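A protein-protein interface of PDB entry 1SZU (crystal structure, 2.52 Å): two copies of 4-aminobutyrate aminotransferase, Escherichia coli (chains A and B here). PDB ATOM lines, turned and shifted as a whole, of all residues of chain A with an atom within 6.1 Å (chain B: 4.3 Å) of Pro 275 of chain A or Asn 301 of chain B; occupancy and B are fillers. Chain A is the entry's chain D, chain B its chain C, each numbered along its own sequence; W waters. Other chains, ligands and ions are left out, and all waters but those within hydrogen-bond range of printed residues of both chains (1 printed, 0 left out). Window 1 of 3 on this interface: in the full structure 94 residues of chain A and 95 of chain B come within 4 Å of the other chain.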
ATOM      1  N   VAL A 108     -23.987  13.575  -4.308  1.00  0.00           N
ATOM      2  CA  VAL A 108     -24.416  12.175  -4.306  1.00  0.00           C
ATOM      3  C   VAL A 108     -23.713  11.512  -3.108  1.00  0.00           C
ATOM      4  O   VAL A 108     -23.454  12.173  -2.101  1.00  0.00           O
ATOM      5  CB  VAL A 108     -24.070  11.460  -5.631  1.00  0.00           C
ATOM      6  CG1 VAL A 108     -24.967  11.989  -6.722  1.00  0.00           C
ATOM      7  CG2 VAL A 108     -22.608  11.687  -6.015  1.00  0.00           C
ATOM      8  N   THR A 109     -23.405  10.227  -3.183  1.00  0.00           N
ATOM      9  CA  THR A 109     -22.742   9.591  -2.047  1.00  0.00           C
ATOM     10  C   THR A 109     -21.403   8.944  -2.393  1.00  0.00           C
ATOM     11  O   THR A 109     -20.485   8.977  -1.577  1.00  0.00           O
ATOM     12  CB  THR A 109     -23.667   8.551  -1.399  1.00  0.00           C
ATOM     13  OG1 THR A 109     -24.941   9.158  -1.150  1.00  0.00           O
ATOM     14  CG2 THR A 109     -23.070   8.022  -0.085  1.00  0.00           C
ATOM     15  N   THR A 110     -21.274   8.397  -3.603  1.00  0.00           N
ATOM     16  CA  THR A 110     -20.030   7.735  -4.006  1.00  0.00           C
ATOM     17  C   THR A 110     -19.408   8.286  -5.294  1.00  0.00           C
ATOM     18  O   THR A 110     -20.101   8.855  -6.141  1.00  0.00           O
ATOM     19  CB  THR A 110     -20.238   6.199  -4.208  1.00  0.00           C
ATOM     20  OG1 THR A 110     -21.114   5.985  -5.318  1.00  0.00           O
ATOM     21  CG2 THR A 110     -20.836   5.543  -2.957  1.00  0.00           C
ATOM     22  N   ALA A 271     -14.752  14.725   2.064  1.00  0.00           N
ATOM     23  CA  ALA A 271     -15.391  14.654   3.374  1.00  0.00           C
ATOM     24  C   ALA A 271     -14.533  14.047   4.496  1.00  0.00           C
ATOM     25  O   ALA A 271     -15.040  13.765   5.573  1.00  0.00           O
ATOM     26  CB  ALA A 271     -16.726  13.926   3.257  1.00  0.00           C
ATOM     27  N   GLY A 273     -13.246  11.071   5.337  1.00  0.00           N
ATOM     28  CA  GLY A 273     -13.568   9.843   6.034  1.00  0.00           C
ATOM     29  C   GLY A 273     -15.055   9.623   6.217  1.00  0.00           C
ATOM     30  O   GLY A 273     -15.470   8.838   7.080  1.00  0.00           O
ATOM     31  N   PHE A 274     -15.867  10.328   5.434  1.00  0.00           N
ATOM     32  CA  PHE A 274     -17.312  10.173   5.517  1.00  0.00           C
ATOM     33  C   PHE A 274     -17.886  10.043   4.111  1.00  0.00           C
ATOM     34  O   PHE A 274     -17.426  10.682   3.178  1.00  0.00           O
ATOM     35  CB  PHE A 274     -17.920  11.334   6.292  1.00  0.00           C
ATOM     36  CG  PHE A 274     -17.456  11.404   7.722  1.00  0.00           C
ATOM     37  CD1 PHE A 274     -16.233  11.981   8.040  1.00  0.00           C
ATOM     38  CD2 PHE A 274     -18.227  10.840   8.745  1.00  0.00           C
ATOM     39  CE1 PHE A 274     -15.771  11.995   9.351  1.00  0.00           C
ATOM     40  CE2 PHE A 274     -17.781  10.844  10.060  1.00  0.00           C
ATOM     41  CZ  PHE A 274     -16.542  11.424  10.368  1.00  0.00           C
ATOM     42  N   PRO A 275     -18.898   9.188   3.941  1.00  0.00           N
ATOM     43  CA  PRO A 275     -19.530   8.941   2.640  1.00  0.00           C
ATOM     44  C   PRO A 275     -20.147  10.164   1.972  1.00  0.00           C
ATOM     45  O   PRO A 275     -21.235  10.589   2.336  1.00  0.00           O
ATOM     46  CB  PRO A 275     -20.582   7.871   2.964  1.00  0.00           C
ATOM     47  CG  PRO A 275     -20.105   7.268   4.239  1.00  0.00           C
ATOM     48  CD  PRO A 275     -19.623   8.468   4.998  1.00  0.00           C
ATOM     49  N   LEU A 276     -19.444  10.696   0.974  1.00  0.00           N
ATOM     50  CA  LEU A 276     -19.894  11.864   0.230  1.00  0.00           C
ATOM     51  C   LEU A 276     -19.185  12.008  -1.109  1.00  0.00           C
ATOM     52  O   LEU A 276     -17.983  11.785  -1.217  1.00  0.00           O
ATOM     53  CB  LEU A 276     -19.639  13.144   1.024  1.00  0.00           C
ATOM     54  CG  LEU A 276     -20.275  14.391   0.370  1.00  0.00           C
ATOM     55  CD1 LEU A 276     -21.776  14.298   0.526  1.00  0.00           C
ATOM     56  CD2 LEU A 276     -19.782  15.664   1.006  1.00  0.00           C
ATOM     57  N   ALA A 277     -19.931  12.396  -2.131  1.00  0.00           N
ATOM     58  CA  ALA A 277     -19.347  12.628  -3.442  1.00  0.00           C
ATOM     59  C   ALA A 277     -20.217  13.682  -4.122  1.00  0.00           C
ATOM     60  O   ALA A 277     -21.264  14.071  -3.594  1.00  0.00           O
ATOM     61  CB  ALA A 277     -19.328  11.353  -4.249  1.00  0.00           C
ATOM     62  N   TYR A 298     -29.409   8.585   0.074  1.00  0.00           N
ATOM     63  CA  TYR A 298     -28.430   9.135   0.994  1.00  0.00           C
ATOM     64  C   TYR A 298     -27.734  10.401   0.506  1.00  0.00           C
ATOM     65  O   TYR A 298     -27.044  11.086   1.285  1.00  0.00           O
ATOM     66  CB  TYR A 298     -27.366   8.077   1.302  1.00  0.00           C
ATOM     67  CG  TYR A 298     -27.873   6.786   1.937  1.00  0.00           C
ATOM     68  CD1 TYR A 298     -28.744   6.810   3.027  1.00  0.00           C
ATOM     69  CD2 TYR A 298     -27.413   5.540   1.490  1.00  0.00           C
ATOM     70  CE1 TYR A 298     -29.138   5.634   3.664  1.00  0.00           C
ATOM     71  CE2 TYR A 298     -27.806   4.355   2.122  1.00  0.00           C
ATOM     72  CZ  TYR A 298     -28.665   4.413   3.210  1.00  0.00           C
ATOM     73  OH  TYR A 298     -29.024   3.252   3.862  1.00  0.00           O
ATOM     74  N   GLY A 300     -25.769  13.495  -0.423  1.00  0.00           N
ATOM     75  CA  GLY A 300     -25.428  14.634   0.411  1.00  0.00           C
ATOM     76  C   GLY A 300     -25.885  14.430   1.840  1.00  0.00           C
ATOM     77  O   GLY A 300     -26.680  15.199   2.390  1.00  0.00           O
ATOM     78  N   ASN A 301     -25.381  13.371   2.445  1.00  0.00           N
ATOM     79  CA  ASN A 301     -25.721  13.048   3.812  1.00  0.00           C
ATOM     80  C   ASN A 301     -25.312  14.189   4.750  1.00  0.00           C
ATOM     81  O   ASN A 301     -24.176  14.700   4.672  1.00  0.00           O
ATOM     82  CB  ASN A 301     -25.015  11.745   4.210  1.00  0.00           C
ATOM     83  CG  ASN A 301     -25.085  11.479   5.688  1.00  0.00           C
ATOM     84  OD1 ASN A 301     -24.198  11.886   6.443  1.00  0.00           O
ATOM     85  ND2 ASN A 301     -26.154  10.807   6.123  1.00  0.00           N
ATOM     86  N   ALA A 304     -22.025  13.864   6.628  1.00  0.00           N
ATOM     87  CA  ALA A 304     -20.909  13.994   5.685  1.00  0.00           C
ATOM     88  C   ALA A 304     -20.731  15.412   5.126  1.00  0.00           C
ATOM     89  O   ALA A 304     -19.615  15.821   4.805  1.00  0.00           O
ATOM     90  CB  ALA A 304     -21.049  12.975   4.534  1.00  0.00           C
ATOM     91  N   SER B  74     -13.447   6.371  11.288  1.00  0.00           N
ATOM     92  CA  SER B  74     -14.622   6.511  10.428  1.00  0.00           C
ATOM     93  C   SER B  74     -14.422   5.883   9.057  1.00  0.00           C
ATOM     94  O   SER B  74     -15.382   5.580   8.364  1.00  0.00           O
ATOM     95  CB  SER B  74     -14.992   7.992  10.252  1.00  0.00           C
ATOM     96  OG  SER B  74     -14.068   8.666   9.407  1.00  0.00           O
ATOM     97  N   TYR B  83     -12.220  -4.270   9.130  1.00  0.00           N
ATOM     98  CA  TYR B  83     -12.637  -3.875  10.458  1.00  0.00           C
ATOM     99  C   TYR B  83     -13.826  -4.724  10.864  1.00  0.00           C
ATOM    100  O   TYR B  83     -14.615  -5.163  10.022  1.00  0.00           O
ATOM    101  CB  TYR B  83     -12.930  -2.354  10.533  1.00  0.00           C
ATOM    102  CG  TYR B  83     -13.619  -1.750   9.324  1.00  0.00           C
ATOM    103  CD1 TYR B  83     -15.009  -1.744   9.218  1.00  0.00           C
ATOM    104  CD2 TYR B  83     -12.872  -1.213   8.272  1.00  0.00           C
ATOM    105  CE1 TYR B  83     -15.635  -1.227   8.101  1.00  0.00           C
ATOM    106  CE2 TYR B  83     -13.493  -0.696   7.136  1.00  0.00           C
ATOM    107  CZ  TYR B  83     -14.878  -0.708   7.053  1.00  0.00           C
ATOM    108  OH  TYR B  83     -15.508  -0.257   5.907  1.00  0.00           O
ATOM    109  N   PRO B 275     -25.428   6.216   5.701  1.00  0.00           N
ATOM    110  CA  PRO B 275     -25.164   5.584   4.407  1.00  0.00           C
ATOM    111  C   PRO B 275     -24.598   4.168   4.388  1.00  0.00           C
ATOM    112  O   PRO B 275     -23.405   3.947   4.640  1.00  0.00           O
ATOM    113  CB  PRO B 275     -24.211   6.573   3.711  1.00  0.00           C
ATOM    114  CG  PRO B 275     -24.319   7.852   4.528  1.00  0.00           C
ATOM    115  CD  PRO B 275     -24.498   7.333   5.926  1.00  0.00           C
ATOM    116  N   LEU B 276     -25.457   3.214   4.044  1.00  0.00           N
ATOM    117  CA  LEU B 276     -25.040   1.832   3.943  1.00  0.00           C
ATOM    118  C   LEU B 276     -26.033   1.004   3.134  1.00  0.00           C
ATOM    119  O   LEU B 276     -27.229   1.291   3.098  1.00  0.00           O
ATOM    120  CB  LEU B 276     -24.869   1.210   5.338  1.00  0.00           C
ATOM    121  CG  LEU B 276     -24.378  -0.250   5.303  1.00  0.00           C
ATOM    122  CD1 LEU B 276     -22.917  -0.319   5.701  1.00  0.00           C
ATOM    123  CD2 LEU B 276     -25.214  -1.098   6.221  1.00  0.00           C
ATOM    124  N   TYR B 298     -16.083   3.657  -0.061  1.00  0.00           N
ATOM    125  CA  TYR B 298     -16.822   3.847   1.189  1.00  0.00           C
ATOM    126  C   TYR B 298     -17.561   2.627   1.711  1.00  0.00           C
ATOM    127  O   TYR B 298     -17.989   2.615   2.876  1.00  0.00           O
ATOM    128  CB  TYR B 298     -17.848   4.977   1.034  1.00  0.00           C
ATOM    129  CG  TYR B 298     -17.270   6.354   0.753  1.00  0.00           C
ATOM    130  CD1 TYR B 298     -16.154   6.836   1.466  1.00  0.00           C
ATOM    131  CD2 TYR B 298     -17.898   7.214  -0.146  1.00  0.00           C
ATOM    132  CE1 TYR B 298     -15.698   8.147   1.295  1.00  0.00           C
ATOM    133  CE2 TYR B 298     -17.450   8.527  -0.329  1.00  0.00           C
ATOM    134  CZ  TYR B 298     -16.354   8.996   0.394  1.00  0.00           C
ATOM    135  OH  TYR B 298     -15.935  10.318   0.226  1.00  0.00           O
ATOM    136  N   ALA B 299     -17.740   1.635   0.837  1.00  0.00           N
ATOM    137  CA  ALA B 299     -18.440   0.393   1.137  1.00  0.00           C
ATOM    138  C   ALA B 299     -18.401  -0.044   2.608  1.00  0.00           C
ATOM    139  O   ALA B 299     -17.344  -0.136   3.224  1.00  0.00           O
ATOM    140  CB  ALA B 299     -17.890  -0.715   0.257  1.00  0.00           C
ATOM    141  N   GLY B 300     -19.573  -0.326   3.153  1.00  0.00           N
ATOM    142  CA  GLY B 300     -19.669  -0.740   4.535  1.00  0.00           C
ATOM    143  C   GLY B 300     -18.895   0.178   5.466  1.00  0.00           C
ATOM    144  O   GLY B 300     -18.051  -0.286   6.250  1.00  0.00           O
ATOM    145  N   ASN B 301     -19.176   1.477   5.366  1.00  0.00           N
ATOM    146  CA  ASN B 301     -18.537   2.483   6.189  1.00  0.00           C
ATOM    147  C   ASN B 301     -18.642   2.131   7.681  1.00  0.00           C
ATOM    148  O   ASN B 301     -19.709   1.773   8.178  1.00  0.00           O
ATOM    149  CB  ASN B 301     -19.197   3.831   5.901  1.00  0.00           C
ATOM    150  CG  ASN B 301     -18.766   4.905   6.865  1.00  0.00           C
ATOM    151  OD1 ASN B 301     -19.330   5.035   7.972  1.00  0.00           O
ATOM    152  ND2 ASN B 301     -17.746   5.683   6.470  1.00  0.00           N
ATOM    153  N   PRO B 302     -17.526   2.230   8.418  1.00  0.00           N
ATOM    154  CA  PRO B 302     -17.488   1.917   9.853  1.00  0.00           C
ATOM    155  C   PRO B 302     -18.655   2.463  10.686  1.00  0.00           C
ATOM    156  O   PRO B 302     -19.318   1.721  11.418  1.00  0.00           O
ATOM    157  CB  PRO B 302     -16.146   2.496  10.290  1.00  0.00           C
ATOM    158  CG  PRO B 302     -15.275   2.207   9.092  1.00  0.00           C
ATOM    159  CD  PRO B 302     -16.185   2.589   7.922  1.00  0.00           C
ATOM    160  N   ILE B 303     -18.904   3.762  10.583  1.00  0.00           N
ATOM    161  CA  ILE B 303     -19.974   4.375  11.353  1.00  0.00           C
ATOM    162  C   ILE B 303     -21.368   3.887  10.977  1.00  0.00           C
ATOM    163  O   ILE B 303     -22.211   3.692  11.844  1.00  0.00           O
ATOM    164  CB  ILE B 303     -19.850   5.899  11.257  1.00  0.00           C
ATOM    165  CG1 ILE B 303     -18.554   6.304  11.970  1.00  0.00           C
ATOM    166  CG2 ILE B 303     -21.080   6.579  11.846  1.00  0.00           C
ATOM    167  CD1 ILE B 303     -18.228   7.725  11.902  1.00  0.00           C
ATOM    168  N   ALA B 304     -21.609   3.666   9.689  1.00  0.00           N
ATOM    169  CA  ALA B 304     -22.912   3.160   9.251  1.00  0.00           C
ATOM    170  C   ALA B 304     -23.083   1.685   9.691  1.00  0.00           C
ATOM    171  O   ALA B 304     -24.198   1.264  10.047  1.00  0.00           O
ATOM    172  CB  ALA B 304     -23.052   3.302   7.718  1.00  0.00           C
ATOM    173  N   CYS B 305     -21.994   0.901   9.675  1.00  0.00           N
ATOM    174  CA  CYS B 305     -22.074  -0.509  10.107  1.00  0.00           C
ATOM    175  C   CYS B 305     -22.545  -0.638  11.567  1.00  0.00           C
ATOM    176  O   CYS B 305     -23.504  -1.372  11.833  1.00  0.00           O
ATOM    177  CB  CYS B 305     -20.727  -1.228   9.970  1.00  0.00           C
ATOM    178  SG  CYS B 305     -20.195  -1.616   8.289  1.00  0.00           S
HETATM  179  O   HOH W   1     -14.753  11.449   2.860  1.00  0.00           O
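OG of Ser 74 of chain B lies within hydrogen-bond range of O of Gly 273 of chain A (2.7 Å). The backbone carbonyl oxygen of Leu 276 of chain B sits at hydrogen-bond distance from the side-chain hydroxyl of Tyr 298 of chain A. The side-chain hydroxyl of Tyr 298 of chain B lies within hydrogen-bond range of the backbone carbonyl oxygen of Phe 274 of chain A, at 3.3 Å. The backbone carbonyl oxygen of Leu 276 of chain A sits at hydrogen-bond distance from the side-chain hydroxyl of Tyr 298 of chain B, 2.9 Å away.
O of Ser 74 of chain B sits at hydrogen-bond distance from ND2 of Asn 301 of chain B. The backbone NH (N) of Ile 303 of chain B sits at hydrogen-bond distance from the side-chain amide oxygen (OD1) of Asn 301 of chain B (2.9 Å). The side-chain amide oxygen of Asn 301 of chain B lies within hydrogen-bond range of the backbone NH of Ala 304 of chain B. The side-chain sulfur of Cys 305 of chain B lies within hydrogen-bond range of the backbone carbonyl oxygen of Asn 301 of chain B (3.4 Å). O of Thr 109 of chain A lies within hydrogen-bond range of N of Leu 276 of chain A (3.2 Å). The backbone NH (N) of Ala 304 of chain A sits at hydrogen-bond distance from the side-chain amide oxygen (OD1) of Asn 301 of chain A (2.9 Å).
Among the printed residues, merely in contact across the chains: Thr 109 of chain A with Tyr 298 of chain B (3.3 Å), Gly 273 of chain A with Asn 301 of chain B (3.9 Å), Phe 274 of chain A with Ser 74 of chain B (3.7 Å), Phe 274 of chain A with Ile 303 of chain B (3.6 Å), Pro 275 of chain A with Pro 275 of chain B (3.9 Å), Pro 275 of chain A with Tyr 298 of chain B (3.6 Å), Pro 275 of chain A with Asn 301 of chain B (3.6 Å), Tyr 298 of chain A with Pro 275 of chain B (3.7 Å) and Asn 301 of chain A with Pro 275 of chain B (3.8 Å).
Pro 275 of chain A touches three residues of chain B. Of chain A, only Gly 273 and Pro 275 come within 4 Å of Asn 301 of chain B. Printed residues of chain B within 4 Å of Phe 274 of chain A: Ser 74 (3.7 Å), Tyr 298 (3.3 Å) and Ile 303 (3.6 Å). Of the printed residues of chain A, Ile 303 of chain B touches Phe 274 (3.6 Å). Of the printed residues of chain A, Pro 275 of chain B touches Pro 275, Tyr 298 and Asn 301. Ala 304 of chain A touches none of the printed residues of chain B. Gly 300 of chain A touches none of the printed residues of chain B.
Of the 13 printed residues of chain A, 7 touch a printed residue of chain B. Hydrophobic or aromatic side chains of chain A that line the printed part of chain B: Phe 274, Pro 275 and Tyr 298. Among the printed residues, 13 pairs touch across the chains.
Pro 275 of chain B touches its own counterpart, Pro 275 of chain A. Pro 275 of chain A touches Tyr 298 of chain B, and with the chains exchanged Tyr 298 of chain A touches Pro 275 of chain B. Pro 275 of chain A touches Asn 301 of chain B, and with the chains exchanged Asn 301 of chain A touches Pro 275 of chain B. Leu 276 of chain A touches Tyr 298 of chain B, and with the chains exchanged Tyr 298 of chain A touches Leu 276 of chain B. 6 positions are printed for both chains. Of the 13 pairs that touch across the chains among the printed residues, 7 have their exchanged pair printed and touching as well.
Water W1 lies within hydrogen-bond range of O of Phe 274 of chain A (2.8 Å), N of Gly 273 of chain A (2.9 Å), OH of Tyr 298 of chain B (3.1 Å) and N of Ala 271 of chain A (3.4 Å).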
